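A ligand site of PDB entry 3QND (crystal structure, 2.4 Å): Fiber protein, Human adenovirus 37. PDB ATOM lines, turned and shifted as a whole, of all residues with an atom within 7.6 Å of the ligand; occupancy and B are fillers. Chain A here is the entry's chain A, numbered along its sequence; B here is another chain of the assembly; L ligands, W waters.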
ATOM      1  N   THR A 139       4.058 -11.390   8.801  1.00  0.00           N
ATOM      2  CA  THR A 139       4.420 -10.561   7.660  1.00  0.00           C
ATOM      3  C   THR A 139       5.943 -10.430   7.573  1.00  0.00           C
ATOM      4  O   THR A 139       6.589  -9.952   8.495  1.00  0.00           O
ATOM      5  CB  THR A 139       3.784  -9.156   7.739  1.00  0.00           C
ATOM      6  OG1 THR A 139       2.364  -9.282   7.933  1.00  0.00           O
ATOM      7  CG2 THR A 139       4.034  -8.358   6.469  1.00  0.00           C
ATOM      8  N   ILE A 140       6.488 -10.877   6.448  1.00  0.00           N
ATOM      9  CA  ILE A 140       7.886 -10.666   6.123  1.00  0.00           C
ATOM     10  C   ILE A 140       8.032  -9.692   4.955  1.00  0.00           C
ATOM     11  O   ILE A 140       7.040  -9.359   4.302  1.00  0.00           O
ATOM     12  CB  ILE A 140       8.660 -11.990   5.872  1.00  0.00           C
ATOM     13  CG1 ILE A 140       7.816 -12.975   5.041  1.00  0.00           C
ATOM     14  CG2 ILE A 140       9.044 -12.621   7.188  1.00  0.00           C
ATOM     15  CD1 ILE A 140       7.867 -12.735   3.539  1.00  0.00           C
ATOM     16  N   TYR A 141       9.255  -9.244   4.706  1.00  0.00           N
ATOM     17  CA  TYR A 141       9.482  -8.170   3.737  1.00  0.00           C
ATOM     18  C   TYR A 141      10.565  -8.531   2.722  1.00  0.00           C
ATOM     19  O   TYR A 141      11.644  -8.985   3.088  1.00  0.00           O
ATOM     20  CB  TYR A 141       9.804  -6.861   4.473  1.00  0.00           C
ATOM     21  CG  TYR A 141       8.659  -6.397   5.344  1.00  0.00           C
ATOM     22  CD1 TYR A 141       8.477  -6.908   6.635  1.00  0.00           C
ATOM     23  CD2 TYR A 141       7.736  -5.463   4.876  1.00  0.00           C
ATOM     24  CE1 TYR A 141       7.412  -6.494   7.429  1.00  0.00           C
ATOM     25  CE2 TYR A 141       6.665  -5.043   5.665  1.00  0.00           C
ATOM     26  CZ  TYR A 141       6.518  -5.570   6.942  1.00  0.00           C
ATOM     27  OH  TYR A 141       5.468  -5.162   7.733  1.00  0.00           O
ATOM     28  N   GLY A 144      14.216  -6.757   2.345  1.00  0.00           N
ATOM     29  CA  GLY A 144      14.335  -6.018   3.598  1.00  0.00           C
ATOM     30  C   GLY A 144      13.689  -4.650   3.537  1.00  0.00           C
ATOM     31  O   GLY A 144      13.901  -3.826   4.417  1.00  0.00           O
ATOM     32  N   LYS A 145      12.903  -4.410   2.488  1.00  0.00           N
ATOM     33  CA  LYS A 145      12.252  -3.120   2.290  1.00  0.00           C
ATOM     34  C   LYS A 145      10.908  -3.066   3.010  1.00  0.00           C
ATOM     35  O   LYS A 145      10.073  -3.954   2.830  1.00  0.00           O
ATOM     36  CB  LYS A 145      12.090  -2.804   0.802  1.00  0.00           C
ATOM     37  CG  LYS A 145      13.420  -2.543   0.083  1.00  0.00           C
ATOM     38  CD  LYS A 145      13.222  -2.297  -1.399  1.00  0.00           C
ATOM     39  CE  LYS A 145      14.564  -2.034  -2.091  1.00  0.00           C
ATOM     40  NZ  LYS A 145      14.400  -1.784  -3.564  1.00  0.00           N
ATOM     41  N   PRO A 146      10.696  -2.016   3.839  1.00  0.00           N
ATOM     42  CA  PRO A 146       9.489  -1.900   4.666  1.00  0.00           C
ATOM     43  C   PRO A 146       8.191  -1.778   3.852  1.00  0.00           C
ATOM     44  O   PRO A 146       7.123  -2.156   4.343  1.00  0.00           O
ATOM     45  CB  PRO A 146       9.746  -0.629   5.487  1.00  0.00           C
ATOM     46  CG  PRO A 146      10.760   0.141   4.718  1.00  0.00           C
ATOM     47  CD  PRO A 146      11.612  -0.879   4.020  1.00  0.00           C
ATOM     48  N   ASP A 147       8.302  -1.262   2.631  1.00  0.00           N
ATOM     49  CA  ASP A 147       7.135  -1.088   1.757  1.00  0.00           C
ATOM     50  C   ASP A 147       6.921  -2.264   0.796  1.00  0.00           C
ATOM     51  O   ASP A 147       6.146  -2.150  -0.161  1.00  0.00           O
ATOM     52  CB  ASP A 147       7.240   0.232   0.987  1.00  0.00           C
ATOM     53  CG  ASP A 147       8.385   0.253  -0.017  1.00  0.00           C
ATOM     54  OD1 ASP A 147       9.344  -0.542   0.136  1.00  0.00           O
ATOM     55  OD2 ASP A 147       8.329   1.071  -0.954  1.00  0.00           O
ATOM     56  N   GLN A 148       7.583  -3.388   1.068  1.00  0.00           N
ATOM     57  CA  GLN A 148       7.421  -4.586   0.247  1.00  0.00           C
ATOM     58  C   GLN A 148       7.027  -5.821   1.074  1.00  0.00           C
ATOM     59  O   GLN A 148       7.765  -6.821   1.103  1.00  0.00           O
ATOM     60  CB  GLN A 148       8.675  -4.839  -0.603  1.00  0.00           C
ATOM     61  CG  GLN A 148       8.841  -3.839  -1.743  1.00  0.00           C
ATOM     62  CD  GLN A 148      10.129  -4.012  -2.533  1.00  0.00           C
ATOM     63  OE1 GLN A 148      11.024  -4.757  -2.140  1.00  0.00           O
ATOM     64  NE2 GLN A 148      10.222  -3.303  -3.657  1.00  0.00           N
ATOM     65  N   PRO A 149       5.847  -5.764   1.739  1.00  0.00           N
ATOM     66  CA  PRO A 149       5.415  -6.874   2.586  1.00  0.00           C
ATOM     67  C   PRO A 149       4.909  -8.084   1.812  1.00  0.00           C
ATOM     68  O   PRO A 149       4.403  -7.951   0.705  1.00  0.00           O
ATOM     69  CB  PRO A 149       4.259  -6.262   3.388  1.00  0.00           C
ATOM     70  CG  PRO A 149       3.697  -5.229   2.499  1.00  0.00           C
ATOM     71  CD  PRO A 149       4.875  -4.655   1.746  1.00  0.00           C
ATOM     72  N   ALA A 150       5.079  -9.256   2.417  1.00  0.00           N
ATOM     73  CA  ALA A 150       4.435 -10.480   1.945  1.00  0.00           C
ATOM     74  C   ALA A 150       3.951 -11.269   3.153  1.00  0.00           C
ATOM     75  O   ALA A 150       4.626 -11.303   4.186  1.00  0.00           O
ATOM     76  CB  ALA A 150       5.391 -11.300   1.101  1.00  0.00           C
ATOM     77  N   LYS A 174       0.220  -6.801  -3.283  1.00  0.00           N
ATOM     78  CA  LYS A 174       0.778  -5.664  -4.018  1.00  0.00           C
ATOM     79  C   LYS A 174       1.312  -6.072  -5.389  1.00  0.00           C
ATOM     80  O   LYS A 174       1.728  -7.216  -5.591  1.00  0.00           O
ATOM     81  CB  LYS A 174       1.904  -5.010  -3.218  1.00  0.00           C
ATOM     82  CG  LYS A 174       1.457  -4.035  -2.158  1.00  0.00           C
ATOM     83  CD  LYS A 174       2.669  -3.400  -1.512  1.00  0.00           C
ATOM     84  CE  LYS A 174       2.330  -2.086  -0.850  1.00  0.00           C
ATOM     85  NZ  LYS A 174       3.541  -1.488  -0.243  1.00  0.00           N
ATOM     86  N   TYR A 176       4.159  -6.039  -7.589  1.00  0.00           N
ATOM     87  CA  TYR A 176       5.603  -5.855  -7.578  1.00  0.00           C
ATOM     88  C   TYR A 176       6.218  -5.947  -8.977  1.00  0.00           C
ATOM     89  O   TYR A 176       5.811  -6.783  -9.783  1.00  0.00           O
ATOM     90  CB  TYR A 176       6.278  -6.850  -6.623  1.00  0.00           C
ATOM     91  CG  TYR A 176       5.886  -6.667  -5.178  1.00  0.00           C
ATOM     92  CD1 TYR A 176       6.078  -5.445  -4.532  1.00  0.00           C
ATOM     93  CD2 TYR A 176       5.310  -7.711  -4.445  1.00  0.00           C
ATOM     94  CE1 TYR A 176       5.710  -5.260  -3.212  1.00  0.00           C
ATOM     95  CE2 TYR A 176       4.953  -7.539  -3.114  1.00  0.00           C
ATOM     96  CZ  TYR A 176       5.152  -6.313  -2.505  1.00  0.00           C
ATOM     97  OH  TYR A 176       4.795  -6.127  -1.194  1.00  0.00           O
ATOM     98  N   TYR B 137      11.517  -7.349  11.225  1.00  0.00           N
ATOM     99  CA  TYR B 137      10.617  -6.211  11.325  1.00  0.00           C
ATOM    100  C   TYR B 137       9.544  -6.465  12.385  1.00  0.00           C
ATOM    101  O   TYR B 137       9.108  -7.609  12.594  1.00  0.00           O
ATOM    102  CB  TYR B 137       9.957  -5.922   9.986  1.00  0.00           C
ATOM    103  CG  TYR B 137      10.761  -5.050   9.046  1.00  0.00           C
ATOM    104  CD1 TYR B 137      11.366  -5.584   7.908  1.00  0.00           C
ATOM    105  CD2 TYR B 137      10.913  -3.680   9.297  1.00  0.00           C
ATOM    106  CE1 TYR B 137      12.102  -4.782   7.036  1.00  0.00           C
ATOM    107  CE2 TYR B 137      11.647  -2.874   8.432  1.00  0.00           C
ATOM    108  CZ  TYR B 137      12.230  -3.426   7.311  1.00  0.00           C
ATOM    109  OH  TYR B 137      12.966  -2.621   6.460  1.00  0.00           O
ATOM    110  N   GLY B 138       9.126  -5.401  13.061  1.00  0.00           N
ATOM    111  CA  GLY B 138       8.071  -5.463  14.060  1.00  0.00           C
ATOM    112  C   GLY B 138       7.428  -4.102  14.273  1.00  0.00           C
ATOM    113  O   GLY B 138       7.996  -3.078  13.877  1.00  0.00           O
ATOM    114  N   THR B 139       6.260  -4.099  14.901  1.00  0.00           N
ATOM    115  CA  THR B 139       5.548  -2.860  15.176  1.00  0.00           C
ATOM    116  C   THR B 139       5.226  -2.735  16.669  1.00  0.00           C
ATOM    117  O   THR B 139       4.567  -3.609  17.247  1.00  0.00           O
ATOM    118  CB  THR B 139       4.257  -2.751  14.323  1.00  0.00           C
ATOM    119  OG1 THR B 139       4.604  -2.707  12.931  1.00  0.00           O
ATOM    120  CG2 THR B 139       3.467  -1.495  14.670  1.00  0.00           C
ATOM    121  N   PRO B 149       1.319   3.610  15.968  1.00  0.00           N
ATOM    122  CA  PRO B 149       2.361   2.630  15.676  1.00  0.00           C
ATOM    123  C   PRO B 149       3.712   3.267  15.334  1.00  0.00           C
ATOM    124  O   PRO B 149       3.763   4.401  14.840  1.00  0.00           O
ATOM    125  CB  PRO B 149       1.824   1.894  14.448  1.00  0.00           C
ATOM    126  CG  PRO B 149       0.975   2.904  13.754  1.00  0.00           C
ATOM    127  CD  PRO B 149       0.365   3.750  14.848  1.00  0.00           C
ATOM    128  N   ALA B 150       4.776   2.532  15.621  1.00  0.00           N
ATOM    129  CA  ALA B 150       6.118   2.877  15.184  1.00  0.00           C
ATOM    130  C   ALA B 150       6.846   1.588  14.836  1.00  0.00           C
ATOM    131  O   ALA B 150       6.801   0.616  15.599  1.00  0.00           O
ATOM    132  CB  ALA B 150       6.868   3.657  16.252  1.00  0.00           C
ATOM    133  N   VAL B 151       7.500   1.573  13.684  1.00  0.00           N
ATOM    134  CA  VAL B 151       8.211   0.397  13.200  1.00  0.00           C
ATOM    135  C   VAL B 151       9.563   0.253  13.888  1.00  0.00           C
ATOM    136  O   VAL B 151      10.370   1.177  13.904  1.00  0.00           O
ATOM    137  CB  VAL B 151       8.393   0.430  11.661  1.00  0.00           C
ATOM    138  CG1 VAL B 151       9.186  -0.792  11.173  1.00  0.00           C
ATOM    139  CG2 VAL B 151       7.040   0.506  10.965  1.00  0.00           C
ATOM    140  N   ILE B 152       9.795  -0.923  14.469  1.00  0.00           N
ATOM    141  CA  ILE B 152      11.105  -1.287  14.995  1.00  0.00           C
ATOM    142  C   ILE B 152      11.781  -2.277  14.047  1.00  0.00           C
ATOM    143  O   ILE B 152      11.249  -3.360  13.760  1.00  0.00           O
ATOM    144  CB  ILE B 152      11.035  -1.813  16.468  1.00  0.00           C
ATOM    145  CG1 ILE B 152      12.418  -2.304  16.925  1.00  0.00           C
ATOM    146  CG2 ILE B 152       9.957  -2.909  16.620  1.00  0.00           C
ATOM    147  CD1 ILE B 152      12.506  -2.619  18.410  1.00  0.00           C
ATOM    148  N   LYS B 153      12.952  -1.888  13.549  1.00  0.00           N
ATOM    149  CA  LYS B 153      13.719  -2.694  12.607  1.00  0.00           C
ATOM    150  C   LYS B 153      14.991  -3.178  13.277  1.00  0.00           C
ATOM    151  O   LYS B 153      15.842  -2.374  13.684  1.00  0.00           O
ATOM    152  CB  LYS B 153      14.036  -1.886  11.342  1.00  0.00           C
ATOM    153  CG  LYS B 153      14.770  -2.664  10.250  1.00  0.00           C
ATOM    154  CD  LYS B 153      15.232  -1.746   9.140  1.00  0.00           C
ATOM    155  CE  LYS B 153      16.045  -2.507   8.102  1.00  0.00           C
ATOM    156  NZ  LYS B 153      16.585  -1.628   7.017  1.00  0.00           N
ATOM    157  N   SER B 171      11.373   3.920  13.623  1.00  0.00           N
ATOM    158  CA  SER B 171      10.852   4.886  12.655  1.00  0.00           C
ATOM    159  C   SER B 171       9.337   4.906  12.642  1.00  0.00           C
ATOM    160  O   SER B 171       8.689   3.945  13.057  1.00  0.00           O
ATOM    161  CB  SER B 171      11.405   4.603  11.251  1.00  0.00           C
ATOM    162  OG  SER B 171      10.632   3.624  10.575  1.00  0.00           O
ATOM    163  N   TRP B 172       8.776   6.020  12.180  1.00  0.00           N
ATOM    164  CA  TRP B 172       7.327   6.195  12.073  1.00  0.00           C
ATOM    165  C   TRP B 172       6.983   7.058  10.863  1.00  0.00           C
ATOM    166  O   TRP B 172       7.790   7.880  10.428  1.00  0.00           O
ATOM    167  CB  TRP B 172       6.742   6.786  13.365  1.00  0.00           C
ATOM    168  CG  TRP B 172       7.356   8.084  13.807  1.00  0.00           C
ATOM    169  CD1 TRP B 172       6.863   9.340  13.587  1.00  0.00           C
ATOM    170  CD2 TRP B 172       8.578   8.267  14.545  1.00  0.00           C
ATOM    171  NE1 TRP B 172       7.687  10.285  14.143  1.00  0.00           N
ATOM    172  CE2 TRP B 172       8.749   9.656  14.730  1.00  0.00           C
ATOM    173  CE3 TRP B 172       9.538   7.391  15.063  1.00  0.00           C
ATOM    174  CZ2 TRP B 172       9.852  10.190  15.411  1.00  0.00           C
ATOM    175  CZ3 TRP B 172      10.631   7.920  15.731  1.00  0.00           C
ATOM    176  CH2 TRP B 172      10.776   9.311  15.906  1.00  0.00           C
ATOM    177  N   SER B 173       5.785   6.847  10.319  1.00  0.00           N
ATOM    178  CA  SER B 173       5.326   7.581   9.135  1.00  0.00           C
ATOM    179  C   SER B 173       4.297   8.653   9.485  1.00  0.00           C
ATOM    180  O   SER B 173       4.228   9.695   8.835  1.00  0.00           O
ATOM    181  CB  SER B 173       4.776   6.624   8.072  1.00  0.00           C
ATOM    182  OG  SER B 173       3.862   5.690   8.634  1.00  0.00           O
ATOM    183  N   LYS B 174       3.497   8.392  10.522  1.00  0.00           N
ATOM    184  CA  LYS B 174       2.456   9.320  10.967  1.00  0.00           C
ATOM    185  C   LYS B 174       3.020  10.616  11.539  1.00  0.00           C
ATOM    186  O   LYS B 174       4.148  10.645  12.045  1.00  0.00           O
ATOM    187  CB  LYS B 174       1.564   8.653  12.009  1.00  0.00           C
ATOM    188  CG  LYS B 174       0.539   7.677  11.439  1.00  0.00           C
ATOM    189  CD  LYS B 174      -0.365   7.172  12.537  1.00  0.00           C
ATOM    190  CE  LYS B 174      -1.563   6.441  11.979  1.00  0.00           C
ATOM    191  NZ  LYS B 174      -2.448   5.943  13.068  1.00  0.00           N
HETATM  192  C1  LIG L   1       3.034  -0.907   3.103  1.00  0.00           C
HETATM  193  C2  LIG L   1       2.499  -0.635   4.495  1.00  0.00           C
HETATM  194  C3  LIG L   1       2.431  -1.932   5.312  1.00  0.00           C
HETATM  195  C4  LIG L   1       3.809  -2.396   5.788  1.00  0.00           C
HETATM  196  C5  LIG L   1       4.554  -1.269   6.499  1.00  0.00           C
HETATM  197  C6  LIG L   1       4.610  -0.033   5.605  1.00  0.00           C
HETATM  198  C7  LIG L   1       5.280   1.158   6.264  1.00  0.00           C
HETATM  199  C8  LIG L   1       5.487   2.330   5.302  1.00  0.00           C
HETATM  200  C9  LIG L   1       6.556   3.289   5.813  1.00  0.00           C
HETATM  201  C10 LIG L   1       6.287  -2.182   8.013  1.00  0.00           C
HETATM  202  C11 LIG L   1       7.741  -2.540   8.098  1.00  0.00           C
HETATM  203  N1  LIG L   1       5.907  -1.699   6.824  1.00  0.00           N
HETATM  204  O1  LIG L   1       3.965  -0.212   2.641  1.00  0.00           O
HETATM  205  O2  LIG L   1       2.497  -1.821   2.432  1.00  0.00           O
HETATM  206  O3  LIG L   1       1.175  -0.121   4.348  1.00  0.00           O
HETATM  207  O4  LIG L   1       3.688  -3.508   6.670  1.00  0.00           O
HETATM  208  O5  LIG L   1       3.291   0.354   5.184  1.00  0.00           O
HETATM  209  O6  LIG L   1       4.494   1.597   7.384  1.00  0.00           O
HETATM  210  O7  LIG L   1       5.850   1.859   3.995  1.00  0.00           O
HETATM  211  O8  LIG L   1       7.838   2.669   5.717  1.00  0.00           O
HETATM  212  O9  LIG L   1       5.526  -2.335   8.962  1.00  0.00           O
HETATM  213  O   HOH W   1       3.490  -0.876  11.031  1.00  0.00           O
HETATM  214  O   HOH W   2       9.174   1.658   7.845  1.00  0.00           O
HETATM  215  O   HOH W   3       6.422  -3.940  11.210  1.00  0.00           O
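The backbone carbonyl oxygen (O) of Pro 146 lies within hydrogen-bond range of a nitrogen (N1) of the ligand, at 2.8 Å.
NZ of Lys 174 of chain A lies within salt-bridge range of O2 of the ligand.
The side-chain hydroxyl of Tyr 141 sits at hydrogen-bond distance from an oxygen (O4) of the ligand (2.7 Å).
The backbone carbonyl oxygen (O) of Pro 149 of chain A sits at hydrogen-bond distance from the side-chain hydroxyl (OH) of Tyr 176, 2.7 Å away.
OH of Tyr 137 of chain B is in hydrogen-bond range of O of Gly 144.
N of Val 151 of chain B lies within hydrogen-bond range of O of Ser 171 of chain B.
NZ of Lys 174 of chain A sits at hydrogen-bond distance from O of Asp 147 (2.7 Å).
CA of Asp 147 touches O1 of the ligand (3.4 Å).
Pro 149 of chain A touches the ligand.
Tyr 137 of chain B touches the ligand (CD2 to C11, 3.6 Å).
Val 151 of chain B touches the ligand (CG2 to O9, 3.8 Å).
Hydrophobic or aromatic side chains within 4 Å of the ligand: Tyr 141, Pro 146, Pro 149 of chain A, Tyr 137 of chain B and Val 151 of chain B.
Water W3 lies within hydrogen-bond range of the side-chain hydroxyl of Thr 139 of chain B (2.8 Å), an oxygen (O9) of the ligand (2.9 Å) and the backbone carbonyl oxygen of Gly 138 of chain B (3.2 Å).
Water W1 bridges OG1 of Thr 139 of chain B (2.9 Å) and O9 of the ligand (3.2 Å).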
